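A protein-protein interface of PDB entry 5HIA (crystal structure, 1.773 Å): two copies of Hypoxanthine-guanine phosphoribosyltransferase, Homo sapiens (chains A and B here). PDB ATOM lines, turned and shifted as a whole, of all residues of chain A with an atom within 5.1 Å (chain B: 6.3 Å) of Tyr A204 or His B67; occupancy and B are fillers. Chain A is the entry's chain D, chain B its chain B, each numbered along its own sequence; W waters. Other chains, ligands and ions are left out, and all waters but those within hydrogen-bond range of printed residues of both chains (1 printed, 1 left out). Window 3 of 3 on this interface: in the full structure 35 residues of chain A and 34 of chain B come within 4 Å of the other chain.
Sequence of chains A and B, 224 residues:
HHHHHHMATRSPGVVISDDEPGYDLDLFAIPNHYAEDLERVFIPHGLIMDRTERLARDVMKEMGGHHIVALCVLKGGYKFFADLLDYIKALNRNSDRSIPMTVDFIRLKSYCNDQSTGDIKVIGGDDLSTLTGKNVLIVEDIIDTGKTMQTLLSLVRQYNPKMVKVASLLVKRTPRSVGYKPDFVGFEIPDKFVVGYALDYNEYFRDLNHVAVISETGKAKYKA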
ATOM      1  N   TYR A  34      -8.454 -20.735  -8.039  1.00  0.00           N
ATOM      2  CA  TYR A  34      -7.154 -21.104  -7.466  1.00  0.00           C
ATOM      3  C   TYR A  34      -6.688 -22.526  -7.832  1.00  0.00           C
ATOM      4  O   TYR A  34      -5.658 -22.993  -7.336  1.00  0.00           O
ATOM      5  CB  TYR A  34      -7.181 -20.957  -5.943  1.00  0.00           C
ATOM      6  CG  TYR A  34      -7.270 -19.517  -5.457  1.00  0.00           C
ATOM      7  CD1 TYR A  34      -6.580 -18.497  -6.101  1.00  0.00           C
ATOM      8  CD2 TYR A  34      -8.031 -19.189  -4.336  1.00  0.00           C
ATOM      9  CE1 TYR A  34      -6.662 -17.175  -5.655  1.00  0.00           C
ATOM     10  CE2 TYR A  34      -8.112 -17.883  -3.878  1.00  0.00           C
ATOM     11  CZ  TYR A  34      -7.431 -16.881  -4.539  1.00  0.00           C
ATOM     12  OH  TYR A  34      -7.511 -15.581  -4.096  1.00  0.00           O
ATOM     13  N   LEU A 199      -4.555 -16.020   5.364  1.00  0.00           N
ATOM     14  CA  LEU A 199      -3.125 -15.826   5.061  1.00  0.00           C
ATOM     15  C   LEU A 199      -2.923 -15.613   3.564  1.00  0.00           C
ATOM     16  O   LEU A 199      -3.446 -16.358   2.746  1.00  0.00           O
ATOM     17  CB  LEU A 199      -2.289 -17.012   5.551  1.00  0.00           C
ATOM     18  CG  LEU A 199      -2.068 -16.961   7.064  1.00  0.00           C
ATOM     19  CD1 LEU A 199      -3.124 -17.779   7.805  1.00  0.00           C
ATOM     20  CD2 LEU A 199      -0.660 -17.410   7.432  1.00  0.00           C
ATOM     21  N   ASP A 200      -2.163 -14.583   3.199  1.00  0.00           N
ATOM     22  CA  ASP A 200      -2.130 -14.150   1.813  1.00  0.00           C
ATOM     23  C   ASP A 200      -0.764 -14.252   1.151  1.00  0.00           C
ATOM     24  O   ASP A 200       0.273 -14.255   1.810  1.00  0.00           O
ATOM     25  CB  ASP A 200      -2.548 -12.673   1.691  1.00  0.00           C
ATOM     26  CG  ASP A 200      -1.460 -11.732   2.173  1.00  0.00           C
ATOM     27  OD1 ASP A 200      -1.043 -11.884   3.339  1.00  0.00           O
ATOM     28  OD2 ASP A 200      -0.996 -10.852   1.398  1.00  0.00           O
ATOM     29  N   TYR A 201      -0.798 -14.210  -0.170  1.00  0.00           N
ATOM     30  CA  TYR A 201       0.379 -13.947  -0.983  1.00  0.00           C
ATOM     31  C   TYR A 201       0.001 -12.752  -1.845  1.00  0.00           C
ATOM     32  O   TYR A 201      -0.859 -12.878  -2.708  1.00  0.00           O
ATOM     33  CB  TYR A 201       0.744 -15.170  -1.823  1.00  0.00           C
ATOM     34  CG  TYR A 201       1.858 -14.932  -2.807  1.00  0.00           C
ATOM     35  CD1 TYR A 201       3.163 -14.728  -2.377  1.00  0.00           C
ATOM     36  CD2 TYR A 201       1.606 -14.910  -4.173  1.00  0.00           C
ATOM     37  CE1 TYR A 201       4.183 -14.523  -3.282  1.00  0.00           C
ATOM     38  CE2 TYR A 201       2.618 -14.693  -5.080  1.00  0.00           C
ATOM     39  CZ  TYR A 201       3.904 -14.508  -4.632  1.00  0.00           C
ATOM     40  OH  TYR A 201       4.914 -14.297  -5.548  1.00  0.00           O
ATOM     41  N   ASN A 202       0.627 -11.599  -1.589  1.00  0.00           N
ATOM     42  CA  ASN A 202       0.296 -10.358  -2.271  1.00  0.00           C
ATOM     43  C   ASN A 202      -1.211 -10.100  -2.323  1.00  0.00           C
ATOM     44  O   ASN A 202      -1.757  -9.735  -3.374  1.00  0.00           O
ATOM     45  CB  ASN A 202       0.890 -10.359  -3.680  1.00  0.00           C
ATOM     46  CG  ASN A 202       2.410 -10.434  -3.663  1.00  0.00           C
ATOM     47  OD1 ASN A 202       3.059  -9.839  -2.798  1.00  0.00           O
ATOM     48  ND2 ASN A 202       2.984 -11.180  -4.606  1.00  0.00           N
ATOM     49  N   GLU A 203      -1.860 -10.313  -1.175  1.00  0.00           N
ATOM     50  CA  GLU A 203      -3.289 -10.048  -0.934  1.00  0.00           C
ATOM     51  C   GLU A 203      -4.234 -11.131  -1.446  1.00  0.00           C
ATOM     52  O   GLU A 203      -5.413 -11.153  -1.060  1.00  0.00           O
ATOM     53  CB  GLU A 203      -3.707  -8.690  -1.518  1.00  0.00           C
ATOM     54  CG  GLU A 203      -3.018  -7.499  -0.860  1.00  0.00           C
ATOM     55  CD  GLU A 203      -3.176  -7.521   0.653  1.00  0.00           C
ATOM     56  OE1 GLU A 203      -4.267  -7.910   1.136  1.00  0.00           O
ATOM     57  OE2 GLU A 203      -2.210  -7.153   1.363  1.00  0.00           O
ATOM     58  N   TYR A 204      -3.720 -12.030  -2.281  1.00  0.00           N
ATOM     59  CA  TYR A 204      -4.510 -13.156  -2.780  1.00  0.00           C
ATOM     60  C   TYR A 204      -4.509 -14.324  -1.809  1.00  0.00           C
ATOM     61  O   TYR A 204      -3.657 -14.390  -0.928  1.00  0.00           O
ATOM     62  CB  TYR A 204      -3.991 -13.621  -4.136  1.00  0.00           C
ATOM     63  CG  TYR A 204      -4.299 -12.640  -5.233  1.00  0.00           C
ATOM     64  CD1 TYR A 204      -5.523 -12.672  -5.885  1.00  0.00           C
ATOM     65  CD2 TYR A 204      -3.375 -11.667  -5.605  1.00  0.00           C
ATOM     66  CE1 TYR A 204      -5.823 -11.768  -6.887  1.00  0.00           C
ATOM     67  CE2 TYR A 204      -3.665 -10.753  -6.610  1.00  0.00           C
ATOM     68  CZ  TYR A 204      -4.893 -10.810  -7.248  1.00  0.00           C
ATOM     69  OH  TYR A 204      -5.200  -9.919  -8.253  1.00  0.00           O
ATOM     70  N   PHE A 205      -5.488 -15.216  -1.991  1.00  0.00           N
ATOM     71  CA  PHE A 205      -5.665 -16.465  -1.238  1.00  0.00           C
ATOM     72  C   PHE A 205      -6.268 -16.276   0.155  1.00  0.00           C
ATOM     73  O   PHE A 205      -6.398 -17.252   0.894  1.00  0.00           O
ATOM     74  CB  PHE A 205      -4.337 -17.247  -1.098  1.00  0.00           C
ATOM     75  CG  PHE A 205      -3.700 -17.624  -2.409  1.00  0.00           C
ATOM     76  CD1 PHE A 205      -4.186 -18.687  -3.159  1.00  0.00           C
ATOM     77  CD2 PHE A 205      -2.604 -16.910  -2.891  1.00  0.00           C
ATOM     78  CE1 PHE A 205      -3.584 -19.040  -4.363  1.00  0.00           C
ATOM     79  CE2 PHE A 205      -1.990 -17.258  -4.104  1.00  0.00           C
ATOM     80  CZ  PHE A 205      -2.485 -18.328  -4.837  1.00  0.00           C
ATOM     81  N   ARG A 206      -6.648 -15.048   0.521  1.00  0.00           N
ATOM     82  CA  ARG A 206      -7.337 -14.857   1.788  1.00  0.00           C
ATOM     83  C   ARG A 206      -8.719 -15.497   1.683  1.00  0.00           C
ATOM     84  O   ARG A 206      -9.239 -15.999   2.675  1.00  0.00           O
ATOM     85  CB  ARG A 206      -7.455 -13.372   2.181  1.00  0.00           C
ATOM     86  CG  ARG A 206      -6.104 -12.651   2.342  1.00  0.00           C
ATOM     87  CD  ARG A 206      -6.213 -11.431   3.247  1.00  0.00           C
ATOM     88  NE  ARG A 206      -5.105 -10.481   3.098  1.00  0.00           N
ATOM     89  CZ  ARG A 206      -4.030 -10.430   3.879  1.00  0.00           C
ATOM     90  NH1 ARG A 206      -3.875 -11.299   4.857  1.00  0.00           N
ATOM     91  NH2 ARG A 206      -3.103  -9.498   3.679  1.00  0.00           N
ATOM     92  N   ASP A 207      -9.279 -15.503   0.468  1.00  0.00           N
ATOM     93  CA  ASP A 207     -10.604 -16.073   0.179  1.00  0.00           C
ATOM     94  C   ASP A 207     -10.542 -17.582  -0.096  1.00  0.00           C
ATOM     95  O   ASP A 207     -10.955 -18.053  -1.157  1.00  0.00           O
ATOM     96  CB  ASP A 207     -11.238 -15.366  -1.027  1.00  0.00           C
ATOM     97  CG  ASP A 207     -10.353 -15.396  -2.251  1.00  0.00           C
ATOM     98  OD1 ASP A 207      -9.105 -15.384  -2.095  1.00  0.00           O
ATOM     99  OD2 ASP A 207     -10.890 -15.444  -3.391  1.00  0.00           O
ATOM    100  N   TYR A 222       0.567 -14.377  -9.286  1.00  0.00           N
ATOM    101  CA  TYR A 222       0.222 -13.286  -8.378  1.00  0.00           C
ATOM    102  C   TYR A 222       1.419 -12.486  -7.865  1.00  0.00           C
ATOM    103  O   TYR A 222       1.279 -11.668  -6.951  1.00  0.00           O
ATOM    104  CB  TYR A 222      -0.571 -13.835  -7.196  1.00  0.00           C
ATOM    105  CG  TYR A 222      -1.794 -14.602  -7.639  1.00  0.00           C
ATOM    106  CD1 TYR A 222      -2.886 -13.944  -8.193  1.00  0.00           C
ATOM    107  CD2 TYR A 222      -1.853 -15.983  -7.504  1.00  0.00           C
ATOM    108  CE1 TYR A 222      -4.004 -14.650  -8.602  1.00  0.00           C
ATOM    109  CE2 TYR A 222      -2.965 -16.697  -7.907  1.00  0.00           C
ATOM    110  CZ  TYR A 222      -4.035 -16.021  -8.458  1.00  0.00           C
ATOM    111  OH  TYR A 222      -5.142 -16.729  -8.866  1.00  0.00           O
ATOM    112  N   MET B  63     -22.063  -9.148  -8.844  1.00  0.00           N
ATOM    113  CA  MET B  63     -20.673  -8.687  -8.781  1.00  0.00           C
ATOM    114  C   MET B  63     -19.642  -9.745  -9.159  1.00  0.00           C
ATOM    115  O   MET B  63     -18.436  -9.468  -9.173  1.00  0.00           O
ATOM    116  CB  MET B  63     -20.362  -8.180  -7.373  1.00  0.00           C
ATOM    117  CG  MET B  63     -21.339  -7.121  -6.863  1.00  0.00           C
ATOM    118  SD  MET B  63     -20.799  -6.380  -5.319  1.00  0.00           S
ATOM    119  CE  MET B  63     -19.458  -5.322  -5.896  1.00  0.00           C
ATOM    120  N   GLY B  64     -20.112 -10.945  -9.484  1.00  0.00           N
ATOM    121  CA  GLY B  64     -19.227 -12.080  -9.648  1.00  0.00           C
ATOM    122  C   GLY B  64     -18.493 -12.174 -10.970  1.00  0.00           C
ATOM    123  O   GLY B  64     -17.755 -13.125 -11.190  1.00  0.00           O
ATOM    124  N   GLY B  65     -18.678 -11.199 -11.853  1.00  0.00           N
ATOM    125  CA  GLY B  65     -18.029 -11.229 -13.156  1.00  0.00           C
ATOM    126  C   GLY B  65     -16.595 -10.730 -13.169  1.00  0.00           C
ATOM    127  O   GLY B  65     -15.877 -10.901 -14.162  1.00  0.00           O
ATOM    128  N   HIS B  66     -16.162 -10.126 -12.070  1.00  0.00           N
ATOM    129  CA  HIS B  66     -14.836  -9.515 -12.014  1.00  0.00           C
ATOM    130  C   HIS B  66     -14.344  -9.483 -10.582  1.00  0.00           C
ATOM    131  O   HIS B  66     -15.149  -9.479  -9.648  1.00  0.00           O
ATOM    132  CB  HIS B  66     -14.875  -8.097 -12.599  1.00  0.00           C
ATOM    133  CG  HIS B  66     -13.527  -7.459 -12.767  1.00  0.00           C
ATOM    134  ND1 HIS B  66     -12.689  -7.754 -13.822  1.00  0.00           N
ATOM    135  CD2 HIS B  66     -12.881  -6.524 -12.025  1.00  0.00           C
ATOM    136  CE1 HIS B  66     -11.584  -7.033 -13.721  1.00  0.00           C
ATOM    137  NE2 HIS B  66     -11.674  -6.282 -12.638  1.00  0.00           N
ATOM    138  N   HIS B  67     -13.023  -9.485 -10.424  1.00  0.00           N
ATOM    139  CA  HIS B  67     -12.367  -9.379  -9.122  1.00  0.00           C
ATOM    140  C   HIS B  67     -13.089  -8.423  -8.166  1.00  0.00           C
ATOM    141  O   HIS B  67     -13.257  -7.244  -8.461  1.00  0.00           O
ATOM    142  CB  HIS B  67     -10.919  -8.923  -9.314  1.00  0.00           C
ATOM    143  CG  HIS B  67     -10.133  -8.828  -8.042  1.00  0.00           C
ATOM    144  ND1 HIS B  67      -8.861  -9.342  -7.923  1.00  0.00           N
ATOM    145  CD2 HIS B  67     -10.426  -8.268  -6.845  1.00  0.00           C
ATOM    146  CE1 HIS B  67      -8.409  -9.112  -6.702  1.00  0.00           C
ATOM    147  NE2 HIS B  67      -9.341  -8.461  -6.029  1.00  0.00           N
ATOM    148  N   ILE B  68     -13.498  -8.950  -7.019  1.00  0.00           N
ATOM    149  CA  ILE B  68     -14.181  -8.166  -5.997  1.00  0.00           C
ATOM    150  C   ILE B  68     -13.192  -7.734  -4.917  1.00  0.00           C
ATOM    151  O   ILE B  68     -12.391  -8.546  -4.457  1.00  0.00           O
ATOM    152  CB  ILE B  68     -15.336  -8.975  -5.352  1.00  0.00           C
ATOM    153  CG1 ILE B  68     -16.408  -9.308  -6.395  1.00  0.00           C
ATOM    154  CG2 ILE B  68     -15.956  -8.216  -4.163  1.00  0.00           C
ATOM    155  CD1 ILE B  68     -17.441 -10.335  -5.917  1.00  0.00           C
ATOM    156  N   VAL B  69     -13.226  -6.460  -4.538  1.00  0.00           N
ATOM    157  CA  VAL B  69     -12.544  -6.026  -3.322  1.00  0.00           C
ATOM    158  C   VAL B  69     -13.609  -5.794  -2.263  1.00  0.00           C
ATOM    159  O   VAL B  69     -14.479  -4.941  -2.405  1.00  0.00           O
ATOM    160  CB  VAL B  69     -11.694  -4.763  -3.516  1.00  0.00           C
ATOM    161  CG1 VAL B  69     -11.009  -4.403  -2.207  1.00  0.00           C
ATOM    162  CG2 VAL B  69     -10.648  -4.966  -4.629  1.00  0.00           C
ATOM    163  N   ILE B  99     -14.545 -16.194  -8.919  1.00  0.00           N
ATOM    164  CA  ILE B  99     -13.720 -15.008  -9.104  1.00  0.00           C
ATOM    165  C   ILE B  99     -12.916 -14.745  -7.831  1.00  0.00           C
ATOM    166  O   ILE B  99     -13.403 -14.985  -6.728  1.00  0.00           O
ATOM    167  CB  ILE B  99     -14.598 -13.768  -9.467  1.00  0.00           C
ATOM    168  CG1 ILE B  99     -13.794 -12.727 -10.247  1.00  0.00           C
ATOM    169  CG2 ILE B  99     -15.272 -13.164  -8.229  1.00  0.00           C
ATOM    170  CD1 ILE B  99     -13.295 -13.225 -11.583  1.00  0.00           C
ATOM    171  N   PRO B 100     -11.677 -14.256  -7.974  1.00  0.00           N
ATOM    172  CA  PRO B 100     -10.933 -13.936  -6.756  1.00  0.00           C
ATOM    173  C   PRO B 100     -11.571 -12.801  -5.952  1.00  0.00           C
ATOM    174  O   PRO B 100     -12.210 -11.891  -6.498  1.00  0.00           O
ATOM    175  CB  PRO B 100      -9.551 -13.524  -7.285  1.00  0.00           C
ATOM    176  CG  PRO B 100      -9.773 -13.180  -8.720  1.00  0.00           C
ATOM    177  CD  PRO B 100     -10.843 -14.111  -9.179  1.00  0.00           C
ATOM    178  N   MET B 101     -11.409 -12.867  -4.639  1.00  0.00           N
ATOM    179  CA  MET B 101     -11.784 -11.754  -3.784  1.00  0.00           C
ATOM    180  C   MET B 101     -10.595 -11.376  -2.927  1.00  0.00           C
ATOM    181  O   MET B 101      -9.872 -12.257  -2.450  1.00  0.00           O
ATOM    182  CB  MET B 101     -12.989 -12.112  -2.910  1.00  0.00           C
ATOM    183  CG  MET B 101     -13.485 -10.949  -2.075  1.00  0.00           C
ATOM    184  SD  MET B 101     -14.968 -11.432  -1.174  1.00  0.00           S
ATOM    185  CE  MET B 101     -15.764 -12.415  -2.412  1.00  0.00           C
ATOM    186  N   THR B 102     -10.361 -10.074  -2.792  1.00  0.00           N
ATOM    187  CA  THR B 102      -9.385  -9.548  -1.857  1.00  0.00           C
ATOM    188  C   THR B 102     -10.134  -8.718  -0.804  1.00  0.00           C
ATOM    189  O   THR B 102     -11.311  -8.389  -0.985  1.00  0.00           O
ATOM    190  CB  THR B 102      -8.289  -8.707  -2.577  1.00  0.00           C
ATOM    191  OG1 THR B 102      -8.892  -7.694  -3.388  1.00  0.00           O
ATOM    192  CG2 THR B 102      -7.448  -9.609  -3.461  1.00  0.00           C
ATOM    193  N   GLY B 133     -10.633   0.124 -11.042  1.00  0.00           N
ATOM    194  CA  GLY B 133     -10.932  -0.933 -11.990  1.00  0.00           C
ATOM    195  C   GLY B 133     -11.500  -2.200 -11.376  1.00  0.00           C
ATOM    196  O   GLY B 133     -11.691  -3.199 -12.076  1.00  0.00           O
ATOM    197  N   LYS B 134     -11.785  -2.166 -10.077  1.00  0.00           N
ATOM    198  CA  LYS B 134     -12.274  -3.356  -9.384  1.00  0.00           C
ATOM    199  C   LYS B 134     -13.760  -3.245  -9.057  1.00  0.00           C
ATOM    200  O   LYS B 134     -14.332  -2.161  -9.103  1.00  0.00           O
ATOM    201  CB  LYS B 134     -11.470  -3.597  -8.103  1.00  0.00           C
ATOM    202  CG  LYS B 134      -9.970  -3.749  -8.344  1.00  0.00           C
ATOM    203  CD  LYS B 134      -9.674  -5.051  -9.067  1.00  0.00           C
ATOM    204  CE  LYS B 134      -8.181  -5.224  -9.339  1.00  0.00           C
ATOM    205  NZ  LYS B 134      -7.381  -5.039  -8.105  1.00  0.00           N
ATOM    206  N   ASN B 135     -14.381  -4.387  -8.773  1.00  0.00           N
ATOM    207  CA  ASN B 135     -15.741  -4.416  -8.226  1.00  0.00           C
ATOM    208  C   ASN B 135     -15.674  -4.286  -6.716  1.00  0.00           C
ATOM    209  O   ASN B 135     -15.249  -5.229  -6.030  1.00  0.00           O
ATOM    210  CB  ASN B 135     -16.462  -5.719  -8.597  1.00  0.00           C
ATOM    211  CG  ASN B 135     -16.833  -5.796 -10.066  1.00  0.00           C
ATOM    212  OD1 ASN B 135     -16.559  -4.877 -10.847  1.00  0.00           O
ATOM    213  ND2 ASN B 135     -17.462  -6.907 -10.453  1.00  0.00           N
ATOM    214  N   VAL B 136     -16.093  -3.142  -6.184  1.00  0.00           N
ATOM    215  CA  VAL B 136     -15.892  -2.877  -4.767  1.00  0.00           C
ATOM    216  C   VAL B 136     -17.161  -3.127  -3.974  1.00  0.00           C
ATOM    217  O   VAL B 136     -18.201  -2.536  -4.273  1.00  0.00           O
ATOM    218  CB  VAL B 136     -15.409  -1.427  -4.537  1.00  0.00           C
ATOM    219  CG1 VAL B 136     -15.299  -1.123  -3.046  1.00  0.00           C
ATOM    220  CG2 VAL B 136     -14.066  -1.215  -5.248  1.00  0.00           C
HETATM  221  O   HOH W   1     -13.619 -15.303  -3.988  1.00  0.00           O
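Among the printed residues, merely in contact across the chains: Glu A203 with Thr B102, Tyr A204 with His B67 and Asp A207 with Pro B100.
N of Met B101 lies within hydrogen-bond range of OD2 of Asp A207, 2.9 Å away.
No position is printed for both chains.
Water W1 lies within hydrogen-bond range of O of Ile B99 (2.8 Å), OD2 of Asp A207 (2.8 Å) and N of Met B101 (3.4 Å).
Of the 11 printed residues of chain A, 3 touch a printed residue of chain B.
Printed residues of chain A that touch a printed residue of chain B: Glu A203, Tyr A204 and Asp A207.
Printed residues of chain B that touch a printed residue of chain A: His B67, Pro B100, Met B101 and Thr B102.
Hydrophobic or aromatic side chains of chain B within 4 Å of the printed part of chain A: His B67 and Met B101.
Among the printed residues, 4 pairs touch across the chains.
Among the printed residues, no Asp or Glu carboxylate lies within 4 Å of a Lys or Arg side-chain nitrogen of the other chain.
The backbone NH (N) of Ile B68 sits at hydrogen-bond distance from the backbone carbonyl oxygen (O) of Pro B100 (3.3 Å).
The backbone carbonyl oxygen (O) of His B67 sits at hydrogen-bond distance from the backbone NH (N) of Asn B135.
OD2 of Asp A200 lies within hydrogen-bond range of N of Glu A203 (2.8 Å).
A ring nitrogen (NE2) of His B67 sits at hydrogen-bond distance from the side-chain hydroxyl (OG1) of Thr B102, at 2.8 Å.
OD1 of Asp A207 lies within hydrogen-bond range of OH of Tyr A34 (2.6 Å).
NH2 of Arg A206 lies within salt-bridge range of OE1 of Glu A203, 3.2 Å away.
Of the printed residues of chain B, Glu A203 touches Thr B102 (3.5 Å).
Printed residues of chain B within 4 Å of Asp A207: Pro B100 and Met B101.
His B67 touches just one residue of chain A: Tyr A204 (3.7 Å).
Val B69 touches none of the printed residues of chain A.
The nearest residue of chain B that does not touch Tyr A204 is Pro B100 (4.1 Å).
The nearest printed residue of chain A that does not touch His B67 is Glu A203 (6.7 Å).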
